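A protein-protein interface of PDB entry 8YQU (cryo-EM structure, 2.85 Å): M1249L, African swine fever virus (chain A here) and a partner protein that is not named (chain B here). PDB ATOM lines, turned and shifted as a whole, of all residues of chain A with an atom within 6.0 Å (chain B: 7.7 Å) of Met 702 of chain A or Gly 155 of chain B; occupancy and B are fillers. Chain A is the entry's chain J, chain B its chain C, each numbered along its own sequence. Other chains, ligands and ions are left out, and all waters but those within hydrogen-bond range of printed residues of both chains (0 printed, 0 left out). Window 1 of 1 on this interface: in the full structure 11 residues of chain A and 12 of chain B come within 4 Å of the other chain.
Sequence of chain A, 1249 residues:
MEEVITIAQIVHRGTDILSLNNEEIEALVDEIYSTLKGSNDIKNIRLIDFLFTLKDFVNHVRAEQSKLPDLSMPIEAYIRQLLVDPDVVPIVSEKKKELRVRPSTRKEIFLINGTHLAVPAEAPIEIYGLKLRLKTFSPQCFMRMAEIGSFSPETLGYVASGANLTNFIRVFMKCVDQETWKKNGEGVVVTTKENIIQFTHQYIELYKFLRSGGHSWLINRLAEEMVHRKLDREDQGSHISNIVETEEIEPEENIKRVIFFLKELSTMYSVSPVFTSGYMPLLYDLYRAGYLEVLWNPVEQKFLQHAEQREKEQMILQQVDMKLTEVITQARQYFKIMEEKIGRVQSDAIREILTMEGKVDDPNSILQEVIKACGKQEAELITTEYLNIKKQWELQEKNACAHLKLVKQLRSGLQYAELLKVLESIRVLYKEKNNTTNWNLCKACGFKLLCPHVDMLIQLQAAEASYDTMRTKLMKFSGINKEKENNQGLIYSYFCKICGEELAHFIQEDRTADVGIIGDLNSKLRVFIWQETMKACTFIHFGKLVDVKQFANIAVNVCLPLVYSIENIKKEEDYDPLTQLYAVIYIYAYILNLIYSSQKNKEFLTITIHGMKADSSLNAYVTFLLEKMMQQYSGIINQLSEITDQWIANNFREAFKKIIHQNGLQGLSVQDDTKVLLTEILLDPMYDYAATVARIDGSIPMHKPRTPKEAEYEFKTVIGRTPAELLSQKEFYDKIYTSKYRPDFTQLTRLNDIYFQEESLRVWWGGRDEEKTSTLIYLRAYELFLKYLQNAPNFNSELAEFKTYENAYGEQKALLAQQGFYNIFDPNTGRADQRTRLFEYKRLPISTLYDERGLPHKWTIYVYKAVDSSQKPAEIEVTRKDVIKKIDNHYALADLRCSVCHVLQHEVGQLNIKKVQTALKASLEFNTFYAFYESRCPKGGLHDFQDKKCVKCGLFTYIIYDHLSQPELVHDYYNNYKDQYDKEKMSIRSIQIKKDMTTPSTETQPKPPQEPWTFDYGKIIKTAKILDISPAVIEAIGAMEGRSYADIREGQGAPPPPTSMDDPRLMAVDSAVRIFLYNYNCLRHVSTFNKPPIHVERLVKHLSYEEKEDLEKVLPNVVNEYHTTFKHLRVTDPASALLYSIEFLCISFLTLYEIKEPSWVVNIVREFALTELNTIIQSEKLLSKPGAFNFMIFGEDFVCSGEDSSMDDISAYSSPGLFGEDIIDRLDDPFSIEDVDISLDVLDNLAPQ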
ATOM      1  N   THR A 692      -3.208 -14.668   5.161  1.00  0.00           N
ATOM      2  CA  THR A 692      -3.815 -13.341   5.140  1.00  0.00           C
ATOM      3  C   THR A 692      -3.004 -12.358   5.973  1.00  0.00           C
ATOM      4  O   THR A 692      -2.759 -11.218   5.549  1.00  0.00           O
ATOM      5  CB  THR A 692      -5.255 -13.411   5.650  1.00  0.00           C
ATOM      6  OG1 THR A 692      -6.026 -14.267   4.797  1.00  0.00           O
ATOM      7  CG2 THR A 692      -5.882 -12.026   5.667  1.00  0.00           C
ATOM      8  N   ARG A 695      -0.054 -11.445   4.058  1.00  0.00           N
ATOM      9  CA  ARG A 695      -0.394 -10.562   2.950  1.00  0.00           C
ATOM     10  C   ARG A 695      -0.594  -9.128   3.415  1.00  0.00           C
ATOM     11  O   ARG A 695      -0.296  -8.191   2.666  1.00  0.00           O
ATOM     12  CB  ARG A 695      -1.656 -11.060   2.246  1.00  0.00           C
ATOM     13  CG  ARG A 695      -1.426 -12.228   1.313  1.00  0.00           C
ATOM     14  CD  ARG A 695      -2.635 -12.491   0.438  1.00  0.00           C
ATOM     15  NE  ARG A 695      -2.428 -13.647  -0.425  1.00  0.00           N
ATOM     16  CZ  ARG A 695      -2.889 -14.864  -0.168  1.00  0.00           C
ATOM     17  NH1 ARG A 695      -3.599 -15.118   0.919  1.00  0.00           N
ATOM     18  NH2 ARG A 695      -2.632 -15.849  -1.022  1.00  0.00           N
ATOM     19  N   ILE A 696      -1.099  -8.939   4.638  1.00  0.00           N
ATOM     20  CA  ILE A 696      -1.400  -7.591   5.116  1.00  0.00           C
ATOM     21  C   ILE A 696      -0.145  -6.723   5.113  1.00  0.00           C
ATOM     22  O   ILE A 696      -0.156  -5.588   4.621  1.00  0.00           O
ATOM     23  CB  ILE A 696      -2.044  -7.647   6.512  1.00  0.00           C
ATOM     24  CG1 ILE A 696      -3.471  -8.186   6.417  1.00  0.00           C
ATOM     25  CG2 ILE A 696      -2.036  -6.273   7.160  1.00  0.00           C
ATOM     26  CD1 ILE A 696      -4.128  -8.405   7.757  1.00  0.00           C
ATOM     27  N   ILE A 700       4.128 -11.819   1.608  1.00  0.00           N
ATOM     28  CA  ILE A 700       3.840 -12.624   0.425  1.00  0.00           C
ATOM     29  C   ILE A 700       2.999 -11.783  -0.530  1.00  0.00           C
ATOM     30  O   ILE A 700       2.328 -10.838  -0.087  1.00  0.00           O
ATOM     31  CB  ILE A 700       3.133 -13.939   0.796  1.00  0.00           C
ATOM     32  CG1 ILE A 700       1.823 -13.661   1.531  1.00  0.00           C
ATOM     33  CG2 ILE A 700       4.039 -14.819   1.634  1.00  0.00           C
ATOM     34  CD1 ILE A 700       1.007 -14.905   1.805  1.00  0.00           C
ATOM     35  N   PRO A 701       3.015 -12.064  -1.833  1.00  0.00           N
ATOM     36  CA  PRO A 701       2.237 -11.246  -2.771  1.00  0.00           C
ATOM     37  C   PRO A 701       0.741 -11.336  -2.502  1.00  0.00           C
ATOM     38  O   PRO A 701       0.232 -12.349  -2.018  1.00  0.00           O
ATOM     39  CB  PRO A 701       2.594 -11.835  -4.140  1.00  0.00           C
ATOM     40  CG  PRO A 701       3.884 -12.557  -3.924  1.00  0.00           C
ATOM     41  CD  PRO A 701       3.813 -13.088  -2.529  1.00  0.00           C
ATOM     42  N   MET A 702       0.039 -10.246  -2.823  1.00  0.00           N
ATOM     43  CA  MET A 702      -1.400 -10.186  -2.585  1.00  0.00           C
ATOM     44  C   MET A 702      -2.164 -11.193  -3.434  1.00  0.00           C
ATOM     45  O   MET A 702      -3.254 -11.628  -3.044  1.00  0.00           O
ATOM     46  CB  MET A 702      -1.916  -8.774  -2.853  1.00  0.00           C
ATOM     47  CG  MET A 702      -1.848  -7.863  -1.647  1.00  0.00           C
ATOM     48  SD  MET A 702      -3.296  -8.075  -0.598  1.00  0.00           S
ATOM     49  CE  MET A 702      -2.757  -7.238   0.885  1.00  0.00           C
ATOM     50  N   HIS A 703      -1.622 -11.572  -4.584  1.00  0.00           N
ATOM     51  CA  HIS A 703      -2.269 -12.538  -5.455  1.00  0.00           C
ATOM     52  C   HIS A 703      -1.849 -13.954  -5.083  1.00  0.00           C
ATOM     53  O   HIS A 703      -0.710 -14.198  -4.676  1.00  0.00           O
ATOM     54  CB  HIS A 703      -1.928 -12.261  -6.919  1.00  0.00           C
ATOM     55  CG  HIS A 703      -0.463 -12.326  -7.219  1.00  0.00           C
ATOM     56  ND1 HIS A 703       0.368 -11.232  -7.110  1.00  0.00           N
ATOM     57  CD2 HIS A 703       0.320 -13.355  -7.619  1.00  0.00           C
ATOM     58  CE1 HIS A 703       1.599 -11.583  -7.435  1.00  0.00           C
ATOM     59  NE2 HIS A 703       1.598 -12.866  -7.746  1.00  0.00           N
ATOM     60  N   LYS A 704      -2.787 -14.886  -5.220  1.00  0.00           N
ATOM     61  CA  LYS A 704      -2.490 -16.281  -4.946  1.00  0.00           C
ATOM     62  C   LYS A 704      -1.470 -16.806  -5.956  1.00  0.00           C
ATOM     63  O   LYS A 704      -1.401 -16.319  -7.087  1.00  0.00           O
ATOM     64  CB  LYS A 704      -3.764 -17.119  -4.996  1.00  0.00           C
ATOM     65  CG  LYS A 704      -4.692 -16.887  -3.817  1.00  0.00           C
ATOM     66  CD  LYS A 704      -5.924 -17.773  -3.893  1.00  0.00           C
ATOM     67  CE  LYS A 704      -6.756 -17.659  -2.627  1.00  0.00           C
ATOM     68  NZ  LYS A 704      -7.267 -16.276  -2.424  1.00  0.00           N
ATOM     69  N   GLU B  81      -7.458 -14.458 -11.177  1.00  0.00           N
ATOM     70  CA  GLU B  81      -6.097 -14.699 -10.707  1.00  0.00           C
ATOM     71  C   GLU B  81      -5.693 -13.732  -9.601  1.00  0.00           C
ATOM     72  O   GLU B  81      -4.858 -14.073  -8.755  1.00  0.00           O
ATOM     73  CB  GLU B  81      -5.117 -14.600 -11.877  1.00  0.00           C
ATOM     74  CG  GLU B  81      -5.102 -13.239 -12.559  1.00  0.00           C
ATOM     75  CD  GLU B  81      -3.973 -13.094 -13.560  1.00  0.00           C
ATOM     76  OE1 GLU B  81      -3.246 -14.085 -13.787  1.00  0.00           O
ATOM     77  OE2 GLU B  81      -3.811 -11.989 -14.119  1.00  0.00           O
ATOM     78  N   ASP B  82      -6.267 -12.532  -9.585  1.00  0.00           N
ATOM     79  CA  ASP B  82      -5.878 -11.502  -8.631  1.00  0.00           C
ATOM     80  C   ASP B  82      -6.960 -11.148  -7.622  1.00  0.00           C
ATOM     81  O   ASP B  82      -6.626 -10.735  -6.510  1.00  0.00           O
ATOM     82  CB  ASP B  82      -5.459 -10.224  -9.374  1.00  0.00           C
ATOM     83  CG  ASP B  82      -4.213 -10.422 -10.212  1.00  0.00           C
ATOM     84  OD1 ASP B  82      -3.327 -11.194  -9.790  1.00  0.00           O
ATOM     85  OD2 ASP B  82      -4.120  -9.808 -11.295  1.00  0.00           O
ATOM     86  N   SER B  83      -8.235 -11.291  -7.973  1.00  0.00           N
ATOM     87  CA  SER B  83      -9.328 -10.950  -7.064  1.00  0.00           C
ATOM     88  C   SER B  83      -9.435 -12.029  -5.996  1.00  0.00           C
ATOM     89  O   SER B  83     -10.055 -13.073  -6.207  1.00  0.00           O
ATOM     90  CB  SER B  83     -10.634 -10.803  -7.834  1.00  0.00           C
ATOM     91  OG  SER B  83     -10.515  -9.831  -8.857  1.00  0.00           O
ATOM     92  N   THR B  84      -8.829 -11.779  -4.837  1.00  0.00           N
ATOM     93  CA  THR B  84      -8.806 -12.751  -3.753  1.00  0.00           C
ATOM     94  C   THR B  84      -9.969 -12.601  -2.781  1.00  0.00           C
ATOM     95  O   THR B  84     -10.097 -13.426  -1.870  1.00  0.00           O
ATOM     96  CB  THR B  84      -7.488 -12.648  -2.979  1.00  0.00           C
ATOM     97  OG1 THR B  84      -7.252 -11.283  -2.613  1.00  0.00           O
ATOM     98  CG2 THR B  84      -6.332 -13.148  -3.827  1.00  0.00           C
ATOM     99  N   ASP B  85     -10.810 -11.583  -2.942  1.00  0.00           N
ATOM    100  CA  ASP B  85     -11.916 -11.384  -2.015  1.00  0.00           C
ATOM    101  C   ASP B  85     -12.954 -12.486  -2.184  1.00  0.00           C
ATOM    102  O   ASP B  85     -13.323 -12.841  -3.307  1.00  0.00           O
ATOM    103  CB  ASP B  85     -12.560 -10.019  -2.229  1.00  0.00           C
ATOM    104  CG  ASP B  85     -13.573  -9.684  -1.153  1.00  0.00           C
ATOM    105  OD1 ASP B  85     -13.155  -9.301  -0.041  1.00  0.00           O
ATOM    106  OD2 ASP B  85     -14.785  -9.820  -1.412  1.00  0.00           O
ATOM    107  N   SER B 115      -8.271  -2.518  -6.591  1.00  0.00           N
ATOM    108  CA  SER B 115      -8.323  -2.231  -5.164  1.00  0.00           C
ATOM    109  C   SER B 115      -7.465  -3.241  -4.414  1.00  0.00           C
ATOM    110  O   SER B 115      -7.682  -4.453  -4.529  1.00  0.00           O
ATOM    111  CB  SER B 115      -9.762  -2.266  -4.654  1.00  0.00           C
ATOM    112  OG  SER B 115     -10.521  -1.201  -5.199  1.00  0.00           O
ATOM    113  N   LEU B 116      -6.503  -2.735  -3.648  1.00  0.00           N
ATOM    114  CA  LEU B 116      -5.634  -3.539  -2.802  1.00  0.00           C
ATOM    115  C   LEU B 116      -5.842  -3.128  -1.351  1.00  0.00           C
ATOM    116  O   LEU B 116      -5.861  -1.934  -1.035  1.00  0.00           O
ATOM    117  CB  LEU B 116      -4.161  -3.357  -3.190  1.00  0.00           C
ATOM    118  CG  LEU B 116      -3.555  -4.146  -4.358  1.00  0.00           C
ATOM    119  CD1 LEU B 116      -3.570  -5.636  -4.078  1.00  0.00           C
ATOM    120  CD2 LEU B 116      -4.244  -3.838  -5.682  1.00  0.00           C
ATOM    121  N   ASN B 117      -5.992  -4.113  -0.470  1.00  0.00           N
ATOM    122  CA  ASN B 117      -6.295  -3.868   0.941  1.00  0.00           C
ATOM    123  C   ASN B 117      -5.095  -4.292   1.784  1.00  0.00           C
ATOM    124  O   ASN B 117      -4.998  -5.444   2.212  1.00  0.00           O
ATOM    125  CB  ASN B 117      -7.562  -4.608   1.362  1.00  0.00           C
ATOM    126  CG  ASN B 117      -8.115  -4.110   2.681  1.00  0.00           C
ATOM    127  OD1 ASN B 117      -7.592  -3.166   3.270  1.00  0.00           O
ATOM    128  ND2 ASN B 117      -9.180  -4.745   3.153  1.00  0.00           N
ATOM    129  N   ASN B 118      -4.193  -3.348   2.038  1.00  0.00           N
ATOM    130  CA  ASN B 118      -3.006  -3.587   2.847  1.00  0.00           C
ATOM    131  C   ASN B 118      -3.242  -3.337   4.331  1.00  0.00           C
ATOM    132  O   ASN B 118      -2.301  -3.449   5.122  1.00  0.00           O
ATOM    133  CB  ASN B 118      -1.849  -2.712   2.361  1.00  0.00           C
ATOM    134  CG  ASN B 118      -1.253  -3.199   1.059  1.00  0.00           C
ATOM    135  OD1 ASN B 118      -1.610  -4.264   0.560  1.00  0.00           O
ATOM    136  ND2 ASN B 118      -0.335  -2.420   0.501  1.00  0.00           N
ATOM    137  N   SER B 119      -4.465  -2.999   4.724  1.00  0.00           N
ATOM    138  CA  SER B 119      -4.787  -2.660   6.100  1.00  0.00           C
ATOM    139  C   SER B 119      -5.393  -3.861   6.814  1.00  0.00           C
ATOM    140  O   SER B 119      -5.603  -4.927   6.229  1.00  0.00           O
ATOM    141  CB  SER B 119      -5.747  -1.466   6.154  1.00  0.00           C
ATOM    142  OG  SER B 119      -7.003  -1.796   5.586  1.00  0.00           O
ATOM    143  N   CYS B 120      -5.672  -3.672   8.102  1.00  0.00           N
ATOM    144  CA  CYS B 120      -6.251  -4.708   8.944  1.00  0.00           C
ATOM    145  C   CYS B 120      -7.751  -4.531   9.145  1.00  0.00           C
ATOM    146  O   CYS B 120      -8.340  -5.227   9.977  1.00  0.00           O
ATOM    147  CB  CYS B 120      -5.544  -4.742  10.300  1.00  0.00           C
ATOM    148  SG  CYS B 120      -3.806  -5.225  10.221  1.00  0.00           S
ATOM    149  N   GLU B 121      -8.378  -3.620   8.407  1.00  0.00           N
ATOM    150  CA  GLU B 121      -9.804  -3.362   8.523  1.00  0.00           C
ATOM    151  C   GLU B 121     -10.457  -3.414   7.150  1.00  0.00           C
ATOM    152  O   GLU B 121      -9.798  -3.223   6.123  1.00  0.00           O
ATOM    153  CB  GLU B 121     -10.072  -2.002   9.181  1.00  0.00           C
ATOM    154  CG  GLU B 121      -9.679  -0.803   8.331  1.00  0.00           C
ATOM    155  CD  GLU B 121      -8.217  -0.431   8.480  1.00  0.00           C
ATOM    156  OE1 GLU B 121      -7.436  -1.256   8.998  1.00  0.00           O
ATOM    157  OE2 GLU B 121      -7.846   0.691   8.077  1.00  0.00           O
ATOM    158  N   VAL B 122     -11.764  -3.689   7.144  1.00  0.00           N
ATOM    159  CA  VAL B 122     -12.512  -3.759   5.896  1.00  0.00           C
ATOM    160  C   VAL B 122     -12.462  -2.409   5.199  1.00  0.00           C
ATOM    161  O   VAL B 122     -12.788  -1.372   5.793  1.00  0.00           O
ATOM    162  CB  VAL B 122     -13.959  -4.196   6.169  1.00  0.00           C
ATOM    163  CG1 VAL B 122     -14.767  -4.210   4.883  1.00  0.00           C
ATOM    164  CG2 VAL B 122     -13.983  -5.560   6.838  1.00  0.00           C
ATOM    165  N   LEU B 152     -13.810  -4.748   0.839  1.00  0.00           N
ATOM    166  CA  LEU B 152     -12.815  -5.810   0.880  1.00  0.00           C
ATOM    167  C   LEU B 152     -12.469  -6.145   2.321  1.00  0.00           C
ATOM    168  O   LEU B 152     -12.249  -5.244   3.141  1.00  0.00           O
ATOM    169  CB  LEU B 152     -11.544  -5.404   0.132  1.00  0.00           C
ATOM    170  CG  LEU B 152     -11.646  -5.156  -1.369  1.00  0.00           C
ATOM    171  CD1 LEU B 152     -10.319  -4.651  -1.905  1.00  0.00           C
ATOM    172  CD2 LEU B 152     -12.076  -6.416  -2.096  1.00  0.00           C
ATOM    173  N   GLN B 153     -12.412  -7.441   2.617  1.00  0.00           N
ATOM    174  CA  GLN B 153     -11.903  -7.914   3.888  1.00  0.00           C
ATOM    175  C   GLN B 153     -10.402  -7.647   3.967  1.00  0.00           C
ATOM    176  O   GLN B 153      -9.746  -7.456   2.939  1.00  0.00           O
ATOM    177  CB  GLN B 153     -12.190  -9.407   4.042  1.00  0.00           C
ATOM    178  CG  GLN B 153     -13.666  -9.763   3.987  1.00  0.00           C
ATOM    179  CD  GLN B 153     -14.449  -9.185   5.148  1.00  0.00           C
ATOM    180  OE1 GLN B 153     -14.010  -9.241   6.296  1.00  0.00           O
ATOM    181  NE2 GLN B 153     -15.615  -8.624   4.852  1.00  0.00           N
ATOM    182  N   PRO B 154      -9.837  -7.601   5.174  1.00  0.00           N
ATOM    183  CA  PRO B 154      -8.398  -7.336   5.297  1.00  0.00           C
ATOM    184  C   PRO B 154      -7.572  -8.365   4.538  1.00  0.00           C
ATOM    185  O   PRO B 154      -7.841  -9.567   4.591  1.00  0.00           O
ATOM    186  CB  PRO B 154      -8.153  -7.417   6.808  1.00  0.00           C
ATOM    187  CG  PRO B 154      -9.472  -7.117   7.418  1.00  0.00           C
ATOM    188  CD  PRO B 154     -10.488  -7.708   6.491  1.00  0.00           C
ATOM    189  N   GLY B 155      -6.558  -7.878   3.826  1.00  0.00           N
ATOM    190  CA  GLY B 155      -5.680  -8.750   3.075  1.00  0.00           C
ATOM    191  C   GLY B 155      -6.251  -9.294   1.788  1.00  0.00           C
ATOM    192  O   GLY B 155      -5.706 -10.259   1.243  1.00  0.00           O
ATOM    193  N   LYS B 156      -7.330  -8.710   1.278  1.00  0.00           N
ATOM    194  CA  LYS B 156      -7.962  -9.155   0.045  1.00  0.00           C
ATOM    195  C   LYS B 156      -7.743  -8.122  -1.056  1.00  0.00           C
ATOM    196  O   LYS B 156      -7.170  -7.052  -0.835  1.00  0.00           O
ATOM    197  CB  LYS B 156      -9.451  -9.420   0.272  1.00  0.00           C
ATOM    198  CG  LYS B 156      -9.729 -10.442   1.359  1.00  0.00           C
ATOM    199  CD  LYS B 156      -9.143 -11.796   1.002  1.00  0.00           C
ATOM    200  CE  LYS B 156      -9.441 -12.826   2.077  1.00  0.00           C
ATOM    201  NZ  LYS B 156      -8.878 -14.160   1.736  1.00  0.00           N
ATOM    202  N   SER B 157      -8.208  -8.454  -2.258  1.00  0.00           N
ATOM    203  CA  SER B 157      -7.992  -7.604  -3.419  1.00  0.00           C
ATOM    204  C   SER B 157      -9.154  -7.763  -4.387  1.00  0.00           C
ATOM    205  O   SER B 157      -9.893  -8.750  -4.346  1.00  0.00           O
ATOM    206  CB  SER B 157      -6.671  -7.940  -4.119  1.00  0.00           C
ATOM    207  OG  SER B 157      -5.589  -7.892  -3.207  1.00  0.00           O
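The side-chain hydroxyl (OG) of Ser 157 of chain B is in hydrogen-bond range of the side-chain sulfur (SD) of Met 702 of chain A (3.5 Å).
The backbone carbonyl oxygen (O) of Ile 696 of chain A lies close to the backbone carbonyl oxygen (O) of Asn 118 of chain B, 3.1 Å away.
O of Gly 155 of chain B lies close to SD of Met 702 of chain A, 3.7 Å away.
The backbone NH (N) of Asp 85 of chain B lies within hydrogen-bond range of the backbone carbonyl oxygen (O) of Ser 157 of chain B, 3.3 Å away.
OG of Ser 119 of chain B is in hydrogen-bond range of OD1 of Asn 117 of chain B (2.8 Å).
N of Gly 155 of chain B sits at hydrogen-bond distance from O of Asn 117 of chain B (3.3 Å).
N of Asn 117 of chain B sits at hydrogen-bond distance from O of Lys 156 of chain B, at 3.2 Å.
The side-chain hydroxyl of Ser 119 of chain B sits at hydrogen-bond distance from the backbone carbonyl oxygen of Glu 121 of chain B (3.2 Å).
The backbone carbonyl oxygen (O) of Met 702 of chain A is in hydrogen-bond range of the guanidinium group (NE) of Arg 695 of chain A (3.4 Å).
CG2 of Thr 692 of chain A touches O of Pro 154 of chain B, 3.3 Å away.
Arg 695 of chain A touches Gly 155 of chain B.
Ile 696 of chain A touches Ser 119 of chain B.
Cys 120 of chain B touches Ile 696 of chain A.
O of Met 702 of chain A touches CG2 of Thr 84 of chain B (3.5 Å).
CG of Met 702 of chain A touches CD1 of Leu 116 of chain B (3.7 Å).
Met 702 of chain A touches Asn 118 of chain B (CE to OD1, 3.2 Å).
His 703 of chain A touches Glu 81 of chain B (CB to O, 3.9 Å).
His 703 of chain A touches Asp 82 of chain B (CB to OD1, 3.4 Å).
NZ of Lys 704 of chain A touches CG2 of Thr 84 of chain B (3.6 Å).
Of the printed residues of chain B, Met 702 of chain A touches Thr 84 (3.5 Å), Leu 116 (3.7 Å), Asn 117 (3.2 Å), Asn 118 (3.2 Å), Gly 155 (3.7 Å) and Ser 157 (3.5 Å).
Of the printed residues of chain A, Gly 155 of chain B touches Arg 695 and Met 702.
Of the printed residues of chain B, Thr 692 of chain A touches Pro 154.
Of the printed residues of chain A, Asp 82 of chain B touches His 703.
Of the printed residues of chain B, Lys 704 of chain A touches Thr 84.
Ile 700 of chain A touches none of the printed residues of chain B.
The nearest printed residue of chain A that does not touch Pro 154 of chain B is Ile 696 of chain A (4.3 Å).
Of the 8 printed residues of chain A, 6 touch a printed residue of chain B.
Printed residues of chain A that touch a printed residue of chain B: Thr 692, Arg 695, Ile 696, Met 702, His 703 and Lys 704.
Of the 19 printed residues of chain B, 11 touch a printed residue of chain A.
Hydrophobic or aromatic side chains of chain B within 4 Å of the printed part of chain A: Leu 116.
Among the printed residues, 14 pairs touch across the chains.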
